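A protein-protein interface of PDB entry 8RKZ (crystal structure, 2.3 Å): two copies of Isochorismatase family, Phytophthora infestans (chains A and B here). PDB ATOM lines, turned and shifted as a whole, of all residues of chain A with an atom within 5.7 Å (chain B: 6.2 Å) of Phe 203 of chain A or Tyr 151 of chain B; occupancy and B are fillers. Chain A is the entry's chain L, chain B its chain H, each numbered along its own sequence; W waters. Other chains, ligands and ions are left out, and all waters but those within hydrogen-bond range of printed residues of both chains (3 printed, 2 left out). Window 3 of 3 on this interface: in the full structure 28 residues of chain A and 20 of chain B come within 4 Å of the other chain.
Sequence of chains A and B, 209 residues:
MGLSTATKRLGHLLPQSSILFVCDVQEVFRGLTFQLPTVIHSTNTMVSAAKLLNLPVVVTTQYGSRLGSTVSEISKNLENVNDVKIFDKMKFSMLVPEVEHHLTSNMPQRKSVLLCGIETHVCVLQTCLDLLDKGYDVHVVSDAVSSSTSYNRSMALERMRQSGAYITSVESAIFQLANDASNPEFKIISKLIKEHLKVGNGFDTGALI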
ATOM      1  N   PHE A  34      22.045 -10.044  -7.098  1.00  0.00           N
ATOM      2  CA  PHE A  34      21.877 -10.608  -8.430  1.00  0.00           C
ATOM      3  C   PHE A  34      23.121 -11.388  -8.845  1.00  0.00           C
ATOM      4  O   PHE A  34      24.208 -10.817  -8.974  1.00  0.00           O
ATOM      5  CB  PHE A  34      21.586  -9.476  -9.418  1.00  0.00           C
ATOM      6  CG  PHE A  34      21.375  -9.930 -10.823  1.00  0.00           C
ATOM      7  CD1 PHE A  34      20.336 -10.791 -11.138  1.00  0.00           C
ATOM      8  CD2 PHE A  34      22.204  -9.479 -11.840  1.00  0.00           C
ATOM      9  CE1 PHE A  34      20.132 -11.208 -12.442  1.00  0.00           C
ATOM     10  CE2 PHE A  34      22.009  -9.889 -13.148  1.00  0.00           C
ATOM     11  CZ  PHE A  34      20.970 -10.753 -13.450  1.00  0.00           C
ATOM     12  N   GLN A  35      22.953 -12.696  -9.054  1.00  0.00           N
ATOM     13  CA  GLN A  35      24.037 -13.581  -9.486  1.00  0.00           C
ATOM     14  C   GLN A  35      25.238 -13.503  -8.543  1.00  0.00           C
ATOM     15  O   GLN A  35      26.389 -13.444  -8.979  1.00  0.00           O
ATOM     16  CB  GLN A  35      24.460 -13.282 -10.929  1.00  0.00           C
ATOM     17  CG  GLN A  35      23.301 -13.205 -11.917  1.00  0.00           C
ATOM     18  CD  GLN A  35      22.634 -14.549 -12.125  1.00  0.00           C
ATOM     19  OE1 GLN A  35      23.240 -15.599 -11.904  1.00  0.00           O
ATOM     20  NE2 GLN A  35      21.377 -14.527 -12.542  1.00  0.00           N
ATOM     21  N   THR A  38      28.146 -16.035  -9.049  1.00  0.00           N
ATOM     22  CA  THR A  38      29.091 -15.643 -10.092  1.00  0.00           C
ATOM     23  C   THR A  38      30.049 -14.570  -9.584  1.00  0.00           C
ATOM     24  O   THR A  38      31.236 -14.579  -9.928  1.00  0.00           O
ATOM     25  CB  THR A  38      28.339 -15.171 -11.339  1.00  0.00           C
ATOM     26  OG1 THR A  38      27.567 -16.259 -11.873  1.00  0.00           O
ATOM     27  CG2 THR A  38      29.317 -14.685 -12.404  1.00  0.00           C
ATOM     28  N   VAL A  39      29.555 -13.647  -8.757  1.00  0.00           N
ATOM     29  CA  VAL A  39      30.422 -12.633  -8.156  1.00  0.00           C
ATOM     30  C   VAL A  39      31.474 -13.286  -7.264  1.00  0.00           C
ATOM     31  O   VAL A  39      32.664 -12.957  -7.335  1.00  0.00           O
ATOM     32  CB  VAL A  39      29.583 -11.608  -7.370  1.00  0.00           C
ATOM     33  CG1 VAL A  39      30.473 -10.753  -6.470  1.00  0.00           C
ATOM     34  CG2 VAL A  39      28.814 -10.729  -8.325  1.00  0.00           C
ATOM     35  N   SER A 142      33.811  -6.593 -14.489  1.00  0.00           N
ATOM     36  CA  SER A 142      32.362  -6.489 -14.654  1.00  0.00           C
ATOM     37  C   SER A 142      31.649  -7.772 -14.244  1.00  0.00           C
ATOM     38  O   SER A 142      30.543  -7.719 -13.693  1.00  0.00           O
ATOM     39  CB  SER A 142      32.020  -6.113 -16.096  1.00  0.00           C
ATOM     40  OG  SER A 142      32.357  -7.153 -16.990  1.00  0.00           O
ATOM     41  N   ASP A 143      32.254  -8.931 -14.499  1.00  0.00           N
ATOM     42  CA  ASP A 143      31.643 -10.176 -14.045  1.00  0.00           C
ATOM     43  C   ASP A 143      32.001 -10.520 -12.602  1.00  0.00           C
ATOM     44  O   ASP A 143      31.740 -11.651 -12.169  1.00  0.00           O
ATOM     45  CB  ASP A 143      32.013 -11.352 -14.963  1.00  0.00           C
ATOM     46  CG  ASP A 143      33.475 -11.353 -15.379  1.00  0.00           C
ATOM     47  OD1 ASP A 143      34.214 -10.412 -15.017  1.00  0.00           O
ATOM     48  OD2 ASP A 143      33.890 -12.329 -16.044  1.00  0.00           O
ATOM     49  N   ALA A 144      32.591  -9.585 -11.852  1.00  0.00           N
ATOM     50  CA  ALA A 144      32.834  -9.775 -10.425  1.00  0.00           C
ATOM     51  C   ALA A 144      32.223  -8.656  -9.586  1.00  0.00           C
ATOM     52  O   ALA A 144      32.611  -8.470  -8.430  1.00  0.00           O
ATOM     53  CB  ALA A 144      34.332  -9.899 -10.140  1.00  0.00           C
ATOM     54  N   VAL A 145      31.285  -7.896 -10.147  1.00  0.00           N
ATOM     55  CA  VAL A 145      30.539  -6.892  -9.399  1.00  0.00           C
ATOM     56  C   VAL A 145      29.059  -7.111  -9.672  1.00  0.00           C
ATOM     57  O   VAL A 145      28.678  -7.576 -10.752  1.00  0.00           O
ATOM     58  CB  VAL A 145      30.947  -5.448  -9.773  1.00  0.00           C
ATOM     59  CG1 VAL A 145      32.367  -5.152  -9.324  1.00  0.00           C
ATOM     60  CG2 VAL A 145      30.788  -5.213 -11.269  1.00  0.00           C
ATOM     61  N   SER A 146      28.220  -6.773  -8.692  1.00  0.00           N
ATOM     62  CA  SER A 146      26.779  -6.901  -8.880  1.00  0.00           C
ATOM     63  C   SER A 146      26.052  -6.153  -7.772  1.00  0.00           C
ATOM     64  O   SER A 146      26.659  -5.680  -6.808  1.00  0.00           O
ATOM     65  CB  SER A 146      26.335  -8.362  -8.915  1.00  0.00           C
ATOM     66  OG  SER A 146      24.947  -8.449  -9.182  1.00  0.00           O
ATOM     67  N   ARG A 153      23.055  -2.749 -11.383  1.00  0.00           N
ATOM     68  CA  ARG A 153      24.363  -3.207 -11.842  1.00  0.00           C
ATOM     69  C   ARG A 153      24.711  -2.603 -13.200  1.00  0.00           C
ATOM     70  O   ARG A 153      25.775  -1.991 -13.364  1.00  0.00           O
ATOM     71  CB  ARG A 153      24.395  -4.736 -11.913  1.00  0.00           C
ATOM     72  CG  ARG A 153      25.696  -5.290 -12.471  1.00  0.00           C
ATOM     73  CD  ARG A 153      25.681  -6.805 -12.580  1.00  0.00           C
ATOM     74  NE  ARG A 153      26.860  -7.300 -13.284  1.00  0.00           N
ATOM     75  CZ  ARG A 153      26.960  -7.390 -14.605  1.00  0.00           C
ATOM     76  NH1 ARG A 153      25.954  -7.058 -15.402  1.00  0.00           N
ATOM     77  NH2 ARG A 153      28.101  -7.815 -15.140  1.00  0.00           N
ATOM     78  N   LEU A 157      27.721   0.233 -14.047  1.00  0.00           N
ATOM     79  CA  LEU A 157      28.868  -0.020 -14.914  1.00  0.00           C
ATOM     80  C   LEU A 157      29.046   1.108 -15.918  1.00  0.00           C
ATOM     81  O   LEU A 157      30.158   1.609 -16.117  1.00  0.00           O
ATOM     82  CB  LEU A 157      28.710  -1.356 -15.640  1.00  0.00           C
ATOM     83  CG  LEU A 157      28.663  -2.612 -14.778  1.00  0.00           C
ATOM     84  CD1 LEU A 157      28.218  -3.819 -15.614  1.00  0.00           C
ATOM     85  CD2 LEU A 157      30.014  -2.847 -14.126  1.00  0.00           C
ATOM     86  N   THR A 168      36.272  -4.104 -17.636  1.00  0.00           N
ATOM     87  CA  THR A 168      36.918  -5.327 -18.091  1.00  0.00           C
ATOM     88  C   THR A 168      36.182  -6.532 -17.508  1.00  0.00           C
ATOM     89  O   THR A 168      35.071  -6.417 -16.977  1.00  0.00           O
ATOM     90  CB  THR A 168      38.408  -5.338 -17.719  1.00  0.00           C
ATOM     91  OG1 THR A 168      39.022  -6.526 -18.241  1.00  0.00           O
ATOM     92  CG2 THR A 168      38.614  -5.287 -16.199  1.00  0.00           C
ATOM     93  N   SER A 169      36.795  -7.704 -17.654  1.00  0.00           N
ATOM     94  CA  SER A 169      36.261  -8.947 -17.120  1.00  0.00           C
ATOM     95  C   SER A 169      37.406  -9.749 -16.520  1.00  0.00           C
ATOM     96  O   SER A 169      38.578  -9.370 -16.620  1.00  0.00           O
ATOM     97  CB  SER A 169      35.534  -9.749 -18.204  1.00  0.00           C
ATOM     98  OG  SER A 169      36.463 -10.338 -19.092  1.00  0.00           O
ATOM     99  N   ASN A 201      28.889 -18.361 -16.632  1.00  0.00           N
ATOM    100  CA  ASN A 201      28.811 -16.962 -16.230  1.00  0.00           C
ATOM    101  C   ASN A 201      27.345 -16.591 -16.030  1.00  0.00           C
ATOM    102  O   ASN A 201      26.554 -16.643 -16.976  1.00  0.00           O
ATOM    103  CB  ASN A 201      29.469 -16.078 -17.292  1.00  0.00           C
ATOM    104  CG  ASN A 201      29.503 -14.605 -16.913  1.00  0.00           C
ATOM    105  OD1 ASN A 201      28.850 -14.168 -15.965  1.00  0.00           O
ATOM    106  ND2 ASN A 201      30.277 -13.829 -17.666  1.00  0.00           N
ATOM    107  N   GLY A 202      26.989 -16.207 -14.802  1.00  0.00           N
ATOM    108  CA  GLY A 202      25.616 -15.831 -14.515  1.00  0.00           C
ATOM    109  C   GLY A 202      25.153 -14.576 -15.225  1.00  0.00           C
ATOM    110  O   GLY A 202      23.944 -14.345 -15.331  1.00  0.00           O
ATOM    111  N   PHE A 203      26.082 -13.754 -15.703  1.00  0.00           N
ATOM    112  CA  PHE A 203      25.729 -12.540 -16.423  1.00  0.00           C
ATOM    113  C   PHE A 203      25.651 -12.739 -17.934  1.00  0.00           C
ATOM    114  O   PHE A 203      25.261 -11.810 -18.645  1.00  0.00           O
ATOM    115  CB  PHE A 203      26.730 -11.427 -16.096  1.00  0.00           C
ATOM    116  CG  PHE A 203      26.883 -11.157 -14.620  1.00  0.00           C
ATOM    117  CD1 PHE A 203      25.852 -10.579 -13.899  1.00  0.00           C
ATOM    118  CD2 PHE A 203      28.058 -11.470 -13.963  1.00  0.00           C
ATOM    119  CE1 PHE A 203      25.987 -10.324 -12.550  1.00  0.00           C
ATOM    120  CE2 PHE A 203      28.201 -11.217 -12.614  1.00  0.00           C
ATOM    121  CZ  PHE A 203      27.164 -10.645 -11.905  1.00  0.00           C
ATOM    122  N   ASP A 204      25.994 -13.926 -18.434  1.00  0.00           N
ATOM    123  CA  ASP A 204      26.090 -14.184 -19.873  1.00  0.00           C
ATOM    124  C   ASP A 204      24.727 -14.636 -20.387  1.00  0.00           C
ATOM    125  O   ASP A 204      24.380 -15.817 -20.310  1.00  0.00           O
ATOM    126  CB  ASP A 204      27.166 -15.228 -20.155  1.00  0.00           C
ATOM    127  CG  ASP A 204      27.619 -15.230 -21.604  1.00  0.00           C
ATOM    128  OD1 ASP A 204      27.031 -14.496 -22.428  1.00  0.00           O
ATOM    129  OD2 ASP A 204      28.573 -15.974 -21.918  1.00  0.00           O
ATOM    130  N   THR A 205      23.958 -13.692 -20.922  1.00  0.00           N
ATOM    131  CA  THR A 205      22.637 -13.991 -21.463  1.00  0.00           C
ATOM    132  C   THR A 205      22.371 -13.181 -22.730  1.00  0.00           C
ATOM    133  O   THR A 205      23.073 -13.329 -23.733  1.00  0.00           O
ATOM    134  CB  THR A 205      21.524 -13.702 -20.438  1.00  0.00           C
ATOM    135  OG1 THR A 205      21.840 -12.506 -19.716  1.00  0.00           O
ATOM    136  CG2 THR A 205      21.384 -14.862 -19.457  1.00  0.00           C
ATOM    137  N   THR B 149      32.798 -16.683 -25.289  1.00  0.00           N
ATOM    138  CA  THR B 149      31.475 -16.349 -24.785  1.00  0.00           C
ATOM    139  C   THR B 149      31.037 -15.010 -25.357  1.00  0.00           C
ATOM    140  O   THR B 149      31.855 -14.118 -25.602  1.00  0.00           O
ATOM    141  CB  THR B 149      31.429 -16.280 -23.244  1.00  0.00           C
ATOM    142  OG1 THR B 149      32.237 -15.189 -22.784  1.00  0.00           O
ATOM    143  CG2 THR B 149      31.930 -17.578 -22.620  1.00  0.00           C
ATOM    144  N   SER B 150      29.726 -14.879 -25.565  1.00  0.00           N
ATOM    145  CA  SER B 150      29.179 -13.613 -26.040  1.00  0.00           C
ATOM    146  C   SER B 150      29.413 -12.490 -25.035  1.00  0.00           C
ATOM    147  O   SER B 150      29.510 -11.318 -25.423  1.00  0.00           O
ATOM    148  CB  SER B 150      27.687 -13.767 -26.330  1.00  0.00           C
ATOM    149  OG  SER B 150      27.066 -12.503 -26.460  1.00  0.00           O
ATOM    150  N   TYR B 151      29.504 -12.827 -23.748  1.00  0.00           N
ATOM    151  CA  TYR B 151      29.737 -11.808 -22.729  1.00  0.00           C
ATOM    152  C   TYR B 151      31.070 -11.108 -22.954  1.00  0.00           C
ATOM    153  O   TYR B 151      31.148  -9.875 -22.931  1.00  0.00           O
ATOM    154  CB  TYR B 151      29.688 -12.440 -21.336  1.00  0.00           C
ATOM    155  CG  TYR B 151      29.896 -11.455 -20.208  1.00  0.00           C
ATOM    156  CD1 TYR B 151      31.178 -11.098 -19.794  1.00  0.00           C
ATOM    157  CD2 TYR B 151      28.813 -10.888 -19.549  1.00  0.00           C
ATOM    158  CE1 TYR B 151      31.372 -10.192 -18.764  1.00  0.00           C
ATOM    159  CE2 TYR B 151      28.996  -9.984 -18.517  1.00  0.00           C
ATOM    160  CZ  TYR B 151      30.277  -9.643 -18.126  1.00  0.00           C
ATOM    161  OH  TYR B 151      30.465  -8.747 -17.095  1.00  0.00           O
ATOM    162  N   ASN B 152      32.136 -11.877 -23.175  1.00  0.00           N
ATOM    163  CA  ASN B 152      33.445 -11.256 -23.316  1.00  0.00           C
ATOM    164  C   ASN B 152      33.620 -10.562 -24.660  1.00  0.00           C
ATOM    165  O   ASN B 152      34.458  -9.661 -24.773  1.00  0.00           O
ATOM    166  CB  ASN B 152      34.542 -12.290 -23.089  1.00  0.00           C
ATOM    167  CG  ASN B 152      34.932 -12.389 -21.634  1.00  0.00           C
ATOM    168  OD1 ASN B 152      34.904 -11.390 -20.914  1.00  0.00           O
ATOM    169  ND2 ASN B 152      35.288 -13.585 -21.187  1.00  0.00           N
ATOM    170  N   ARG B 153      32.848 -10.945 -25.676  1.00  0.00           N
ATOM    171  CA  ARG B 153      32.899 -10.209 -26.933  1.00  0.00           C
ATOM    172  C   ARG B 153      32.297  -8.819 -26.773  1.00  0.00           C
ATOM    173  O   ARG B 153      32.931  -7.814 -27.122  1.00  0.00           O
ATOM    174  CB  ARG B 153      32.173 -10.989 -28.028  1.00  0.00           C
ATOM    175  CG  ARG B 153      31.987 -10.205 -29.311  1.00  0.00           C
ATOM    176  CD  ARG B 153      31.305 -11.047 -30.379  1.00  0.00           C
ATOM    177  NE  ARG B 153      31.066 -10.273 -31.589  1.00  0.00           N
ATOM    178  CZ  ARG B 153      30.074  -9.405 -31.735  1.00  0.00           C
ATOM    179  NH1 ARG B 153      29.180  -9.211 -30.779  1.00  0.00           N
ATOM    180  NH2 ARG B 153      29.977  -8.716 -32.870  1.00  0.00           N
ATOM    181  N   SER B 154      31.081  -8.741 -26.224  1.00  0.00           N
ATOM    182  CA  SER B 154      30.422  -7.451 -26.052  1.00  0.00           C
ATOM    183  C   SER B 154      31.201  -6.566 -25.094  1.00  0.00           C
ATOM    184  O   SER B 154      31.373  -5.365 -25.345  1.00  0.00           O
ATOM    185  CB  SER B 154      28.991  -7.651 -25.555  1.00  0.00           C
ATOM    186  OG  SER B 154      28.244  -8.448 -26.460  1.00  0.00           O
ATOM    187  N   MET B 155      31.692  -7.148 -23.998  1.00  0.00           N
ATOM    188  CA  MET B 155      32.558  -6.414 -23.082  1.00  0.00           C
ATOM    189  C   MET B 155      33.758  -5.840 -23.822  1.00  0.00           C
ATOM    190  O   MET B 155      34.047  -4.642 -23.724  1.00  0.00           O
ATOM    191  CB  MET B 155      33.000  -7.344 -21.949  1.00  0.00           C
ATOM    192  CG  MET B 155      33.863  -6.728 -20.850  1.00  0.00           C
ATOM    193  SD  MET B 155      35.550  -6.347 -21.346  1.00  0.00           S
ATOM    194  CE  MET B 155      36.156  -8.007 -21.654  1.00  0.00           C
ATOM    195  N   ALA B 156      34.458  -6.682 -24.588  1.00  0.00           N
ATOM    196  CA  ALA B 156      35.680  -6.238 -25.250  1.00  0.00           C
ATOM    197  C   ALA B 156      35.400  -5.144 -26.271  1.00  0.00           C
ATOM    198  O   ALA B 156      36.203  -4.215 -26.423  1.00  0.00           O
ATOM    199  CB  ALA B 156      36.381  -7.419 -25.917  1.00  0.00           C
HETATM  200  O   HOH W   1      31.570 -15.317 -19.881  1.00  0.00           O
HETATM  201  O   HOH W   2      35.756 -13.299 -17.849  1.00  0.00           O
HETATM  202  O   HOH W   3      27.894 -17.015 -24.369  1.00  0.00           O
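Among the printed residues, pairs that only touch across the chains: Asp 204 of chain A with Thr 149 of chain B, Ser 169 of chain A with Met 155 of chain B, Asn 201 of chain A with Tyr 151 of chain B, Phe 203 of chain A with Tyr 151 of chain B, Thr 168 of chain A with Met 155 of chain B and Asp 204 of chain A with Ser 150 of chain B.
The side-chain hydroxyl (OG1) of Thr 149 of chain B lies within hydrogen-bond range of the backbone NH (N) of Asn 152 of chain B, 3.3 Å away.
The backbone carbonyl oxygen (O) of Ser 150 of chain B sits at hydrogen-bond distance from the side-chain hydroxyl (OG) of Ser 154 of chain B (3.3 Å).
The backbone carbonyl oxygen (O) of Ser 142 of chain A lies within hydrogen-bond range of the guanidinium group (NH2) of Arg 153 of chain A.
O of Thr 168 of chain A is in hydrogen-bond range of N of Ser 142 of chain A (2.8 Å).
O of Val 145 of chain A sits at hydrogen-bond distance from NE of Arg 153 of chain A (3.1 Å).
OD1 of Asn 201 of chain A is in hydrogen-bond range of N of Phe 203 of chain A (2.8 Å).
Phe 203 of chain A touches one residue of chain B.
Of chain A, only Ser 142 (2.5 Å), Asp 143 (3.2 Å), Arg 153 (3.2 Å), Asn 201 (3.5 Å), Phe 203 (3.6 Å) and Asp 204 (3.3 Å) come within 4 Å of Tyr 151 of chain B.
Printed residues of chain A within 4 Å of Met 155 of chain B: Thr 168 (3.7 Å) and Ser 169 (3.5 Å).
Of the printed residues of chain B, Asp 204 of chain A touches Thr 149 (3.2 Å), Ser 150 (3.98 Å) and Tyr 151 (3.3 Å).
Of the printed residues of chain A, Asn 152 of chain B touches Ser 169 (2.6 Å).
Printed residues of chain B within 4 Å of Asp 143 of chain A: Tyr 151.
Arg 153 of chain B touches none of the printed residues of chain A.
The nearest printed residue of chain B that does not touch Phe 203 of chain A is Ser 150 of chain B (7.7 Å).
The nearest residue of chain A that does not touch Tyr 151 of chain B is Ser 169 of chain A (4.2 Å).
Of the 18 printed residues of chain A, 8 touch a printed residue of chain B.
Printed residues of chain A that touch a printed residue of chain B: Ser 142, Asp 143, Arg 153, Thr 168, Ser 169, Asn 201, Phe 203 and Asp 204.
Among the printed residues, 11 pairs touch across the chains.
Among the printed residues, no Asp or Glu carboxylate lies within 4 Å of a Lys or Arg side-chain nitrogen of the other chain.
Water W3 lies within hydrogen-bond range of OD2 of Asp 204 of chain A (2.7 Å) and N of Ser 150 of chain B (3.1 Å).
Water W2 lies within hydrogen-bond range of the side-chain carboxylate of Asp 143 of chain A (2.8 Å), the side-chain hydroxyl of Ser 169 of chain A (3.3 Å) and the side-chain amide nitrogen of Asn 152 of chain B (3.4 Å).
Water W1 lies within hydrogen-bond range of ND2 of Asn 201 of chain A (3.0 Å) and OG1 of Thr 149 of chain B (3.0 Å).
The side-chain hydroxyl (OG) of Ser 142 of chain A sits at hydrogen-bond distance from the side-chain hydroxyl (OH) of Tyr 151 of chain B (2.5 Å).
The side-chain hydroxyl of Tyr 151 of chain B sits at hydrogen-bond distance from the backbone NH of Asp 143 of chain A (3.2 Å).
The guanidinium group (NH2) of Arg 153 of chain A is in hydrogen-bond range of the side-chain hydroxyl (OH) of Tyr 151 of chain B (3.2 Å).
N of Tyr 151 of chain B is in hydrogen-bond range of OD1 of Asp 204 of chain A.
The side-chain amide oxygen (OD1) of Asn 152 of chain B sits at hydrogen-bond distance from the side-chain hydroxyl (OG) of Ser 169 of chain A, at 2.6 Å.
1 position is printed for both chains.
Of the 11 pairs that touch across the chains among the printed residues, none has its exchanged pair printed and touching as well.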
